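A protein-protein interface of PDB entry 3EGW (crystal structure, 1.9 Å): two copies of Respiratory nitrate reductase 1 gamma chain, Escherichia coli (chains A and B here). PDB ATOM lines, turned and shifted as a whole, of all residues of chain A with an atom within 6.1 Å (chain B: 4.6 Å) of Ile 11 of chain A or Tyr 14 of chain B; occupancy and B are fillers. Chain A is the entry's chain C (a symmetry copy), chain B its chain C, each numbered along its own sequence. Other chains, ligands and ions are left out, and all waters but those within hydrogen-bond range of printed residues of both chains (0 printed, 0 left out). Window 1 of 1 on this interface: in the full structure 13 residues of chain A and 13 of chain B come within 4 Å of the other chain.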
ATOM      1  N   MET A   6     -14.727  -2.906 -23.783  1.00  0.00           N
ATOM      2  CA  MET A   6     -13.354  -2.453 -23.920  1.00  0.00           C
ATOM      3  C   MET A   6     -13.115  -1.161 -23.144  1.00  0.00           C
ATOM      4  O   MET A   6     -12.044  -0.961 -22.576  1.00  0.00           O
ATOM      5  CB  MET A   6     -13.002  -2.254 -25.397  1.00  0.00           C
ATOM      6  CG  MET A   6     -13.011  -3.549 -26.197  1.00  0.00           C
ATOM      7  SD  MET A   6     -12.464  -3.321 -27.904  1.00  0.00           S
ATOM      8  CE  MET A   6     -13.913  -2.560 -28.598  1.00  0.00           C
ATOM      9  N   PHE A   7     -14.110  -0.284 -23.109  1.00  0.00           N
ATOM     10  CA  PHE A   7     -13.938   0.956 -22.374  1.00  0.00           C
ATOM     11  C   PHE A   7     -13.702   0.692 -20.887  1.00  0.00           C
ATOM     12  O   PHE A   7     -12.670   1.070 -20.339  1.00  0.00           O
ATOM     13  CB  PHE A   7     -15.156   1.867 -22.511  1.00  0.00           C
ATOM     14  CG  PHE A   7     -15.114   3.044 -21.577  1.00  0.00           C
ATOM     15  CD1 PHE A   7     -14.156   4.041 -21.741  1.00  0.00           C
ATOM     16  CD2 PHE A   7     -15.970   3.109 -20.481  1.00  0.00           C
ATOM     17  CE1 PHE A   7     -14.045   5.085 -20.820  1.00  0.00           C
ATOM     18  CE2 PHE A   7     -15.869   4.149 -19.552  1.00  0.00           C
ATOM     19  CZ  PHE A   7     -14.903   5.137 -19.724  1.00  0.00           C
ATOM     20  N   PHE A   8     -14.661   0.034 -20.243  1.00  0.00           N
ATOM     21  CA  PHE A   8     -14.565  -0.238 -18.811  1.00  0.00           C
ATOM     22  C   PHE A   8     -13.443  -1.158 -18.346  1.00  0.00           C
ATOM     23  O   PHE A   8     -12.945  -1.011 -17.227  1.00  0.00           O
ATOM     24  CB  PHE A   8     -15.888  -0.799 -18.284  1.00  0.00           C
ATOM     25  CG  PHE A   8     -16.968   0.232 -18.127  1.00  0.00           C
ATOM     26  CD1 PHE A   8     -18.079   0.231 -18.964  1.00  0.00           C
ATOM     27  CD2 PHE A   8     -16.885   1.195 -17.124  1.00  0.00           C
ATOM     28  CE1 PHE A   8     -19.097   1.172 -18.804  1.00  0.00           C
ATOM     29  CE2 PHE A   8     -17.898   2.140 -16.954  1.00  0.00           C
ATOM     30  CZ  PHE A   8     -19.005   2.129 -17.796  1.00  0.00           C
ATOM     31  N   PHE A   9     -13.024  -2.092 -19.193  1.00  0.00           N
ATOM     32  CA  PHE A   9     -12.007  -3.046 -18.774  1.00  0.00           C
ATOM     33  C   PHE A   9     -10.640  -2.977 -19.447  1.00  0.00           C
ATOM     34  O   PHE A   9      -9.715  -3.676 -19.038  1.00  0.00           O
ATOM     35  CB  PHE A   9     -12.613  -4.447 -18.867  1.00  0.00           C
ATOM     36  CG  PHE A   9     -13.882  -4.585 -18.075  1.00  0.00           C
ATOM     37  CD1 PHE A   9     -13.853  -4.524 -16.684  1.00  0.00           C
ATOM     38  CD2 PHE A   9     -15.115  -4.665 -18.713  1.00  0.00           C
ATOM     39  CE1 PHE A   9     -15.031  -4.532 -15.941  1.00  0.00           C
ATOM     40  CE2 PHE A   9     -16.302  -4.674 -17.981  1.00  0.00           C
ATOM     41  CZ  PHE A   9     -16.259  -4.605 -16.591  1.00  0.00           C
ATOM     42  N   ASP A  10     -10.509  -2.120 -20.455  1.00  0.00           N
ATOM     43  CA  ASP A  10      -9.244  -1.944 -21.159  1.00  0.00           C
ATOM     44  C   ASP A  10      -8.759  -0.496 -21.089  1.00  0.00           C
ATOM     45  O   ASP A  10      -7.556  -0.238 -21.073  1.00  0.00           O
ATOM     46  CB  ASP A  10      -9.389  -2.332 -22.634  1.00  0.00           C
ATOM     47  CG  ASP A  10      -9.613  -3.817 -22.833  1.00  0.00           C
ATOM     48  OD1 ASP A  10     -10.361  -4.168 -23.766  1.00  0.00           O
ATOM     49  OD2 ASP A  10      -9.034  -4.626 -22.075  1.00  0.00           O
ATOM     50  N   ILE A  11      -9.699   0.445 -21.044  1.00  0.00           N
ATOM     51  CA  ILE A  11      -9.366   1.872 -21.022  1.00  0.00           C
ATOM     52  C   ILE A  11      -9.536   2.523 -19.650  1.00  0.00           C
ATOM     53  O   ILE A  11      -8.591   3.102 -19.102  1.00  0.00           O
ATOM     54  CB  ILE A  11     -10.239   2.639 -22.054  1.00  0.00           C
ATOM     55  CG1 ILE A  11      -9.923   2.134 -23.468  1.00  0.00           C
ATOM     56  CG2 ILE A  11      -9.988   4.143 -21.955  1.00  0.00           C
ATOM     57  CD1 ILE A  11     -10.859   2.679 -24.543  1.00  0.00           C
ATOM     58  N   TYR A  12     -10.743   2.417 -19.109  1.00  0.00           N
ATOM     59  CA  TYR A  12     -11.081   2.989 -17.811  1.00  0.00           C
ATOM     60  C   TYR A  12     -10.090   2.658 -16.688  1.00  0.00           C
ATOM     61  O   TYR A  12      -9.756   3.523 -15.874  1.00  0.00           O
ATOM     62  CB  TYR A  12     -12.491   2.544 -17.410  1.00  0.00           C
ATOM     63  CG  TYR A  12     -13.035   3.236 -16.180  1.00  0.00           C
ATOM     64  CD1 TYR A  12     -13.146   4.627 -16.131  1.00  0.00           C
ATOM     65  CD2 TYR A  12     -13.453   2.502 -15.069  1.00  0.00           C
ATOM     66  CE1 TYR A  12     -13.663   5.271 -15.004  1.00  0.00           C
ATOM     67  CE2 TYR A  12     -13.972   3.135 -13.939  1.00  0.00           C
ATOM     68  CZ  TYR A  12     -14.073   4.519 -13.915  1.00  0.00           C
ATOM     69  OH  TYR A  12     -14.594   5.149 -12.807  1.00  0.00           O
ATOM     70  N   PRO A  13      -9.605   1.404 -16.620  1.00  0.00           N
ATOM     71  CA  PRO A  13      -8.658   1.084 -15.548  1.00  0.00           C
ATOM     72  C   PRO A  13      -7.407   1.955 -15.545  1.00  0.00           C
ATOM     73  O   PRO A  13      -6.840   2.229 -14.489  1.00  0.00           O
ATOM     74  CB  PRO A  13      -8.348  -0.397 -15.781  1.00  0.00           C
ATOM     75  CG  PRO A  13      -8.579  -0.575 -17.248  1.00  0.00           C
ATOM     76  CD  PRO A  13      -9.831   0.235 -17.487  1.00  0.00           C
ATOM     77  N   TYR A  14      -6.977   2.399 -16.720  1.00  0.00           N
ATOM     78  CA  TYR A  14      -5.784   3.236 -16.801  1.00  0.00           C
ATOM     79  C   TYR A  14      -6.097   4.697 -16.507  1.00  0.00           C
ATOM     80  O   TYR A  14      -5.234   5.442 -16.038  1.00  0.00           O
ATOM     81  CB  TYR A  14      -5.114   3.066 -18.166  1.00  0.00           C
ATOM     82  CG  TYR A  14      -4.530   1.681 -18.318  1.00  0.00           C
ATOM     83  CD1 TYR A  14      -3.428   1.287 -17.559  1.00  0.00           C
ATOM     84  CD2 TYR A  14      -5.130   0.736 -19.148  1.00  0.00           C
ATOM     85  CE1 TYR A  14      -2.942  -0.016 -17.616  1.00  0.00           C
ATOM     86  CE2 TYR A  14      -4.653  -0.572 -19.212  1.00  0.00           C
ATOM     87  CZ  TYR A  14      -3.562  -0.941 -18.442  1.00  0.00           C
ATOM     88  OH  TYR A  14      -3.099  -2.237 -18.477  1.00  0.00           O
ATOM     89  N   ILE A  15      -7.331   5.109 -16.774  1.00  0.00           N
ATOM     90  CA  ILE A  15      -7.720   6.477 -16.469  1.00  0.00           C
ATOM     91  C   ILE A  15      -7.780   6.577 -14.942  1.00  0.00           C
ATOM     92  O   ILE A  15      -7.198   7.483 -14.341  1.00  0.00           O
ATOM     93  CB  ILE A  15      -9.106   6.814 -17.053  1.00  0.00           C
ATOM     94  CG1 ILE A  15      -9.031   6.832 -18.581  1.00  0.00           C
ATOM     95  CG2 ILE A  15      -9.587   8.162 -16.524  1.00  0.00           C
ATOM     96  CD1 ILE A  15     -10.366   7.050 -19.262  1.00  0.00           C
ATOM     97  N   ALA A  16      -8.470   5.621 -14.324  1.00  0.00           N
ATOM     98  CA  ALA A  16      -8.619   5.589 -12.874  1.00  0.00           C
ATOM     99  C   ALA A  16      -7.268   5.496 -12.172  1.00  0.00           C
ATOM    100  O   ALA A  16      -7.036   6.178 -11.174  1.00  0.00           O
ATOM    101  CB  ALA A  16      -9.503   4.417 -12.466  1.00  0.00           C
ATOM    102  N   ALA A  18      -4.249   6.383 -13.390  1.00  0.00           N
ATOM    103  CA  ALA A  18      -3.453   7.584 -13.605  1.00  0.00           C
ATOM    104  C   ALA A  18      -3.911   8.682 -12.649  1.00  0.00           C
ATOM    105  O   ALA A  18      -3.089   9.351 -12.023  1.00  0.00           O
ATOM    106  CB  ALA A  18      -3.588   8.059 -15.050  1.00  0.00           C
ATOM    107  N   ASP B  10      -2.817   1.999 -27.304  1.00  0.00           N
ATOM    108  CA  ASP B  10      -4.117   1.654 -26.742  1.00  0.00           C
ATOM    109  C   ASP B  10      -4.216   2.050 -25.268  1.00  0.00           C
ATOM    110  O   ASP B  10      -5.293   2.392 -24.782  1.00  0.00           O
ATOM    111  CB  ASP B  10      -4.370   0.148 -26.854  1.00  0.00           C
ATOM    112  CG  ASP B  10      -4.554  -0.314 -28.285  1.00  0.00           C
ATOM    113  OD1 ASP B  10      -4.116  -1.441 -28.589  1.00  0.00           O
ATOM    114  OD2 ASP B  10      -5.146   0.434 -29.093  1.00  0.00           O
ATOM    115  N   ILE B  11      -3.087   2.006 -24.564  1.00  0.00           N
ATOM    116  CA  ILE B  11      -3.056   2.315 -23.132  1.00  0.00           C
ATOM    117  C   ILE B  11      -2.462   3.686 -22.812  1.00  0.00           C
ATOM    118  O   ILE B  11      -3.109   4.524 -22.174  1.00  0.00           O
ATOM    119  CB  ILE B  11      -2.250   1.227 -22.369  1.00  0.00           C
ATOM    120  CG1 ILE B  11      -2.956  -0.128 -22.513  1.00  0.00           C
ATOM    121  CG2 ILE B  11      -2.108   1.602 -20.894  1.00  0.00           C
ATOM    122  CD1 ILE B  11      -2.153  -1.304 -21.966  1.00  0.00           C
ATOM    123  N   TYR B  12      -1.233   3.899 -23.263  1.00  0.00           N
ATOM    124  CA  TYR B  12      -0.513   5.147 -23.037  1.00  0.00           C
ATOM    125  C   TYR B  12      -1.307   6.414 -23.377  1.00  0.00           C
ATOM    126  O   TYR B  12      -1.253   7.402 -22.638  1.00  0.00           O
ATOM    127  CB  TYR B  12       0.800   5.127 -23.827  1.00  0.00           C
ATOM    128  CG  TYR B  12       1.731   6.278 -23.515  1.00  0.00           C
ATOM    129  CD1 TYR B  12       2.181   6.502 -22.212  1.00  0.00           C
ATOM    130  CD2 TYR B  12       2.175   7.137 -24.522  1.00  0.00           C
ATOM    131  CE1 TYR B  12       3.053   7.553 -21.920  1.00  0.00           C
ATOM    132  CE2 TYR B  12       3.047   8.189 -24.241  1.00  0.00           C
ATOM    133  CZ  TYR B  12       3.481   8.390 -22.938  1.00  0.00           C
ATOM    134  OH  TYR B  12       4.350   9.421 -22.656  1.00  0.00           O
ATOM    135  N   PRO B  13      -2.055   6.412 -24.494  1.00  0.00           N
ATOM    136  CA  PRO B  13      -2.815   7.623 -24.823  1.00  0.00           C
ATOM    137  C   PRO B  13      -3.794   8.053 -23.735  1.00  0.00           C
ATOM    138  O   PRO B  13      -4.053   9.243 -23.566  1.00  0.00           O
ATOM    139  CB  PRO B  13      -3.513   7.257 -26.136  1.00  0.00           C
ATOM    140  CG  PRO B  13      -3.632   5.768 -26.065  1.00  0.00           C
ATOM    141  CD  PRO B  13      -2.296   5.355 -25.491  1.00  0.00           C
ATOM    142  N   TYR B  14      -4.332   7.094 -22.991  1.00  0.00           N
ATOM    143  CA  TYR B  14      -5.279   7.425 -21.932  1.00  0.00           C
ATOM    144  C   TYR B  14      -4.572   7.847 -20.652  1.00  0.00           C
ATOM    145  O   TYR B  14      -5.118   8.612 -19.855  1.00  0.00           O
ATOM    146  CB  TYR B  14      -6.231   6.253 -21.693  1.00  0.00           C
ATOM    147  CG  TYR B  14      -7.150   6.045 -22.874  1.00  0.00           C
ATOM    148  CD1 TYR B  14      -8.138   6.980 -23.178  1.00  0.00           C
ATOM    149  CD2 TYR B  14      -6.975   4.966 -23.739  1.00  0.00           C
ATOM    150  CE1 TYR B  14      -8.925   6.852 -24.321  1.00  0.00           C
ATOM    151  CE2 TYR B  14      -7.755   4.828 -24.885  1.00  0.00           C
ATOM    152  CZ  TYR B  14      -8.724   5.775 -25.171  1.00  0.00           C
ATOM    153  OH  TYR B  14      -9.482   5.663 -26.314  1.00  0.00           O
ATOM    154  N   ILE B  15      -3.355   7.354 -20.452  1.00  0.00           N
ATOM    155  CA  ILE B  15      -2.595   7.753 -19.277  1.00  0.00           C
ATOM    156  C   ILE B  15      -2.207   9.219 -19.494  1.00  0.00           C
ATOM    157  O   ILE B  15      -2.421  10.068 -18.626  1.00  0.00           O
ATOM    158  CB  ILE B  15      -1.315   6.909 -19.118  1.00  0.00           C
ATOM    159  CG1 ILE B  15      -1.690   5.463 -18.785  1.00  0.00           C
ATOM    160  CG2 ILE B  15      -0.428   7.498 -18.026  1.00  0.00           C
ATOM    161  CD1 ILE B  15      -0.507   4.520 -18.711  1.00  0.00           C
ATOM    162  N   ALA B  16      -1.657   9.506 -20.672  1.00  0.00           N
ATOM    163  CA  ALA B  16      -1.231  10.856 -21.017  1.00  0.00           C
ATOM    164  C   ALA B  16      -2.395  11.841 -20.972  1.00  0.00           C
ATOM    165  O   ALA B  16      -2.251  12.955 -20.469  1.00  0.00           O
ATOM    166  CB  ALA B  16      -0.592  10.864 -22.400  1.00  0.00           C
ATOM    167  N   GLY B  17      -3.544  11.421 -21.499  1.00  0.00           N
ATOM    168  CA  GLY B  17      -4.722  12.270 -21.511  1.00  0.00           C
ATOM    169  C   GLY B  17      -5.283  12.546 -20.127  1.00  0.00           C
ATOM    170  O   GLY B  17      -5.712  13.667 -19.832  1.00  0.00           O
ATOM    171  N   ALA B  18      -5.293  11.528 -19.274  1.00  0.00           N
ATOM    172  CA  ALA B  18      -5.804  11.690 -17.919  1.00  0.00           C
ATOM    173  C   ALA B  18      -4.913  12.658 -17.147  1.00  0.00           C
ATOM    174  O   ALA B  18      -5.406  13.554 -16.462  1.00  0.00           O
ATOM    175  CB  ALA B  18      -5.853  10.340 -17.207  1.00  0.00           C
ATOM    176  N   SER B 165     -10.382   6.816 -33.004  1.00  0.00           N
ATOM    177  CA  SER B 165     -10.747   5.705 -32.128  1.00  0.00           C
ATOM    178  C   SER B 165     -10.395   6.078 -30.692  1.00  0.00           C
ATOM    179  O   SER B 165     -11.166   5.836 -29.763  1.00  0.00           O
ATOM    180  CB  SER B 165      -9.982   4.437 -32.518  1.00  0.00           C
ATOM    181  OG  SER B 165     -10.346   3.988 -33.809  1.00  0.00           O
ATOM    182  N   VAL B 166      -9.219   6.673 -30.520  1.00  0.00           N
ATOM    183  CA  VAL B 166      -8.753   7.083 -29.202  1.00  0.00           C
ATOM    184  C   VAL B 166      -9.650   8.137 -28.554  1.00  0.00           C
ATOM    185  O   VAL B 166     -10.056   7.979 -27.401  1.00  0.00           O
ATOM    186  CB  VAL B 166      -7.308   7.638 -29.264  1.00  0.00           C
ATOM    187  CG1 VAL B 166      -6.926   8.268 -27.919  1.00  0.00           C
ATOM    188  CG2 VAL B 166      -6.337   6.520 -29.606  1.00  0.00           C
ATOM    189  N   PHE B 169     -13.033   6.875 -27.425  1.00  0.00           N
ATOM    190  CA  PHE B 169     -12.901   5.743 -26.516  1.00  0.00           C
ATOM    191  C   PHE B 169     -13.306   4.384 -27.083  1.00  0.00           C
ATOM    192  O   PHE B 169     -13.924   3.572 -26.385  1.00  0.00           O
ATOM    193  CB  PHE B 169     -13.675   6.022 -25.223  1.00  0.00           C
ATOM    194  CG  PHE B 169     -13.237   7.278 -24.524  1.00  0.00           C
ATOM    195  CD1 PHE B 169     -13.639   8.527 -24.992  1.00  0.00           C
ATOM    196  CD2 PHE B 169     -12.381   7.216 -23.432  1.00  0.00           C
ATOM    197  CE1 PHE B 169     -13.188   9.699 -24.382  1.00  0.00           C
ATOM    198  CE2 PHE B 169     -11.924   8.381 -22.815  1.00  0.00           C
ATOM    199  CZ  PHE B 169     -12.329   9.625 -23.292  1.00  0.00           C
ATOM    200  N   HIS B 170     -12.956   4.140 -28.346  1.00  0.00           N
ATOM    201  CA  HIS B 170     -13.245   2.861 -29.003  1.00  0.00           C
ATOM    202  C   HIS B 170     -11.994   2.000 -28.902  1.00  0.00           C
ATOM    203  O   HIS B 170     -10.961   2.346 -29.468  1.00  0.00           O
ATOM    204  CB  HIS B 170     -13.572   3.053 -30.489  1.00  0.00           C
ATOM    205  CG  HIS B 170     -15.009   3.354 -30.768  1.00  0.00           C
ATOM    206  ND1 HIS B 170     -15.597   4.558 -30.444  1.00  0.00           N
ATOM    207  CD2 HIS B 170     -15.976   2.608 -31.352  1.00  0.00           C
ATOM    208  CE1 HIS B 170     -16.864   4.542 -30.819  1.00  0.00           C
ATOM    209  NE2 HIS B 170     -17.120   3.371 -31.373  1.00  0.00           N
ATOM    210  N   GLY B 171     -12.084   0.878 -28.196  1.00  0.00           N
ATOM    211  CA  GLY B 171     -10.928   0.010 -28.046  1.00  0.00           C
ATOM    212  C   GLY B 171     -10.402  -0.549 -29.357  1.00  0.00           C
ATOM    213  O   GLY B 171     -11.112  -0.570 -30.362  1.00  0.00           O
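OH of Tyr 14 of chain B lies within hydrogen-bond range of O of Val 166 of chain B (2.6 Å). The backbone carbonyl oxygen (O) of Phe 7 of chain A sits at hydrogen-bond distance from the backbone NH (N) of Tyr 12 of chain A, at 2.7 Å. O of Met 6 of chain A is in hydrogen-bond range of N of Ile 11 of chain A, 3.1 Å away.
Among the printed residues, pairs that only touch across the chains: Met 6 of chain A with Gly 171 of chain B, Phe 7 of chain A with Phe 169 of chain B, Ile 11 of chain A with Tyr 14 of chain B, Ile 11 of chain A with Phe 169 of chain B, Tyr 14 of chain A with Ile 11 of chain B and Ala 18 of chain A with Ala 18 of chain B.
Printed residues of chain B within 4 Å of Met 6 of chain A: Gly 171 (3.7 Å). Ile 11 of chain A touches just these residues of chain B: Tyr 14 and Phe 169. Printed residues of chain B within 4 Å of Tyr 14 of chain A: Ile 11 (3.5 Å). Asp 10 of chain B touches none of the printed residues of chain A. Tyr 14 of chain B touches one residue of chain A. Ala 16 of chain B touches none of the printed residues of chain A. Of the printed residues of chain A, Phe 169 of chain B touches Phe 7 (3.8 Å) and Ile 11 (3.7 Å). Printed residues of chain A within 4 Å of Gly 171 of chain B: Met 6. The nearest residue of chain A that does not touch Tyr 14 of chain B is Ile 15 of chain A (4.2 Å). The nearest printed residue of chain B that does not touch Tyr 14 of chain A is Ile 15 of chain B (4.2 Å).
Of the 12 printed residues of chain A, 5 touch a printed residue of chain B. Hydrophobic or aromatic side chains of chain A that line the printed part of chain B: Met 6, Phe 7, Ile 11, Tyr 14 and Ala 18. Of the 14 printed residues of chain B, 5 touch a printed residue of chain A. Printed residues of chain B that touch a printed residue of chain A: Ile 11, Tyr 14, Ala 18, Phe 169 and Gly 171. Among the printed residues, no Asp or Glu carboxylate lies within 4 Å of a Lys or Arg side-chain nitrogen of the other chain.
Ile 11 of chain A touches Tyr 14 of chain B, and with the chains exchanged Tyr 14 of chain A touches Ile 11 of chain B. Ala 18 of chain B touches its own counterpart, Ala 18 of chain A. Positions printed for both chains: 10, 11, 12, 13, 14, 15, 16 and 18. Of the 6 pairs that touch across the chains among the printed residues, 3 have their exchanged pair printed and touching as well.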
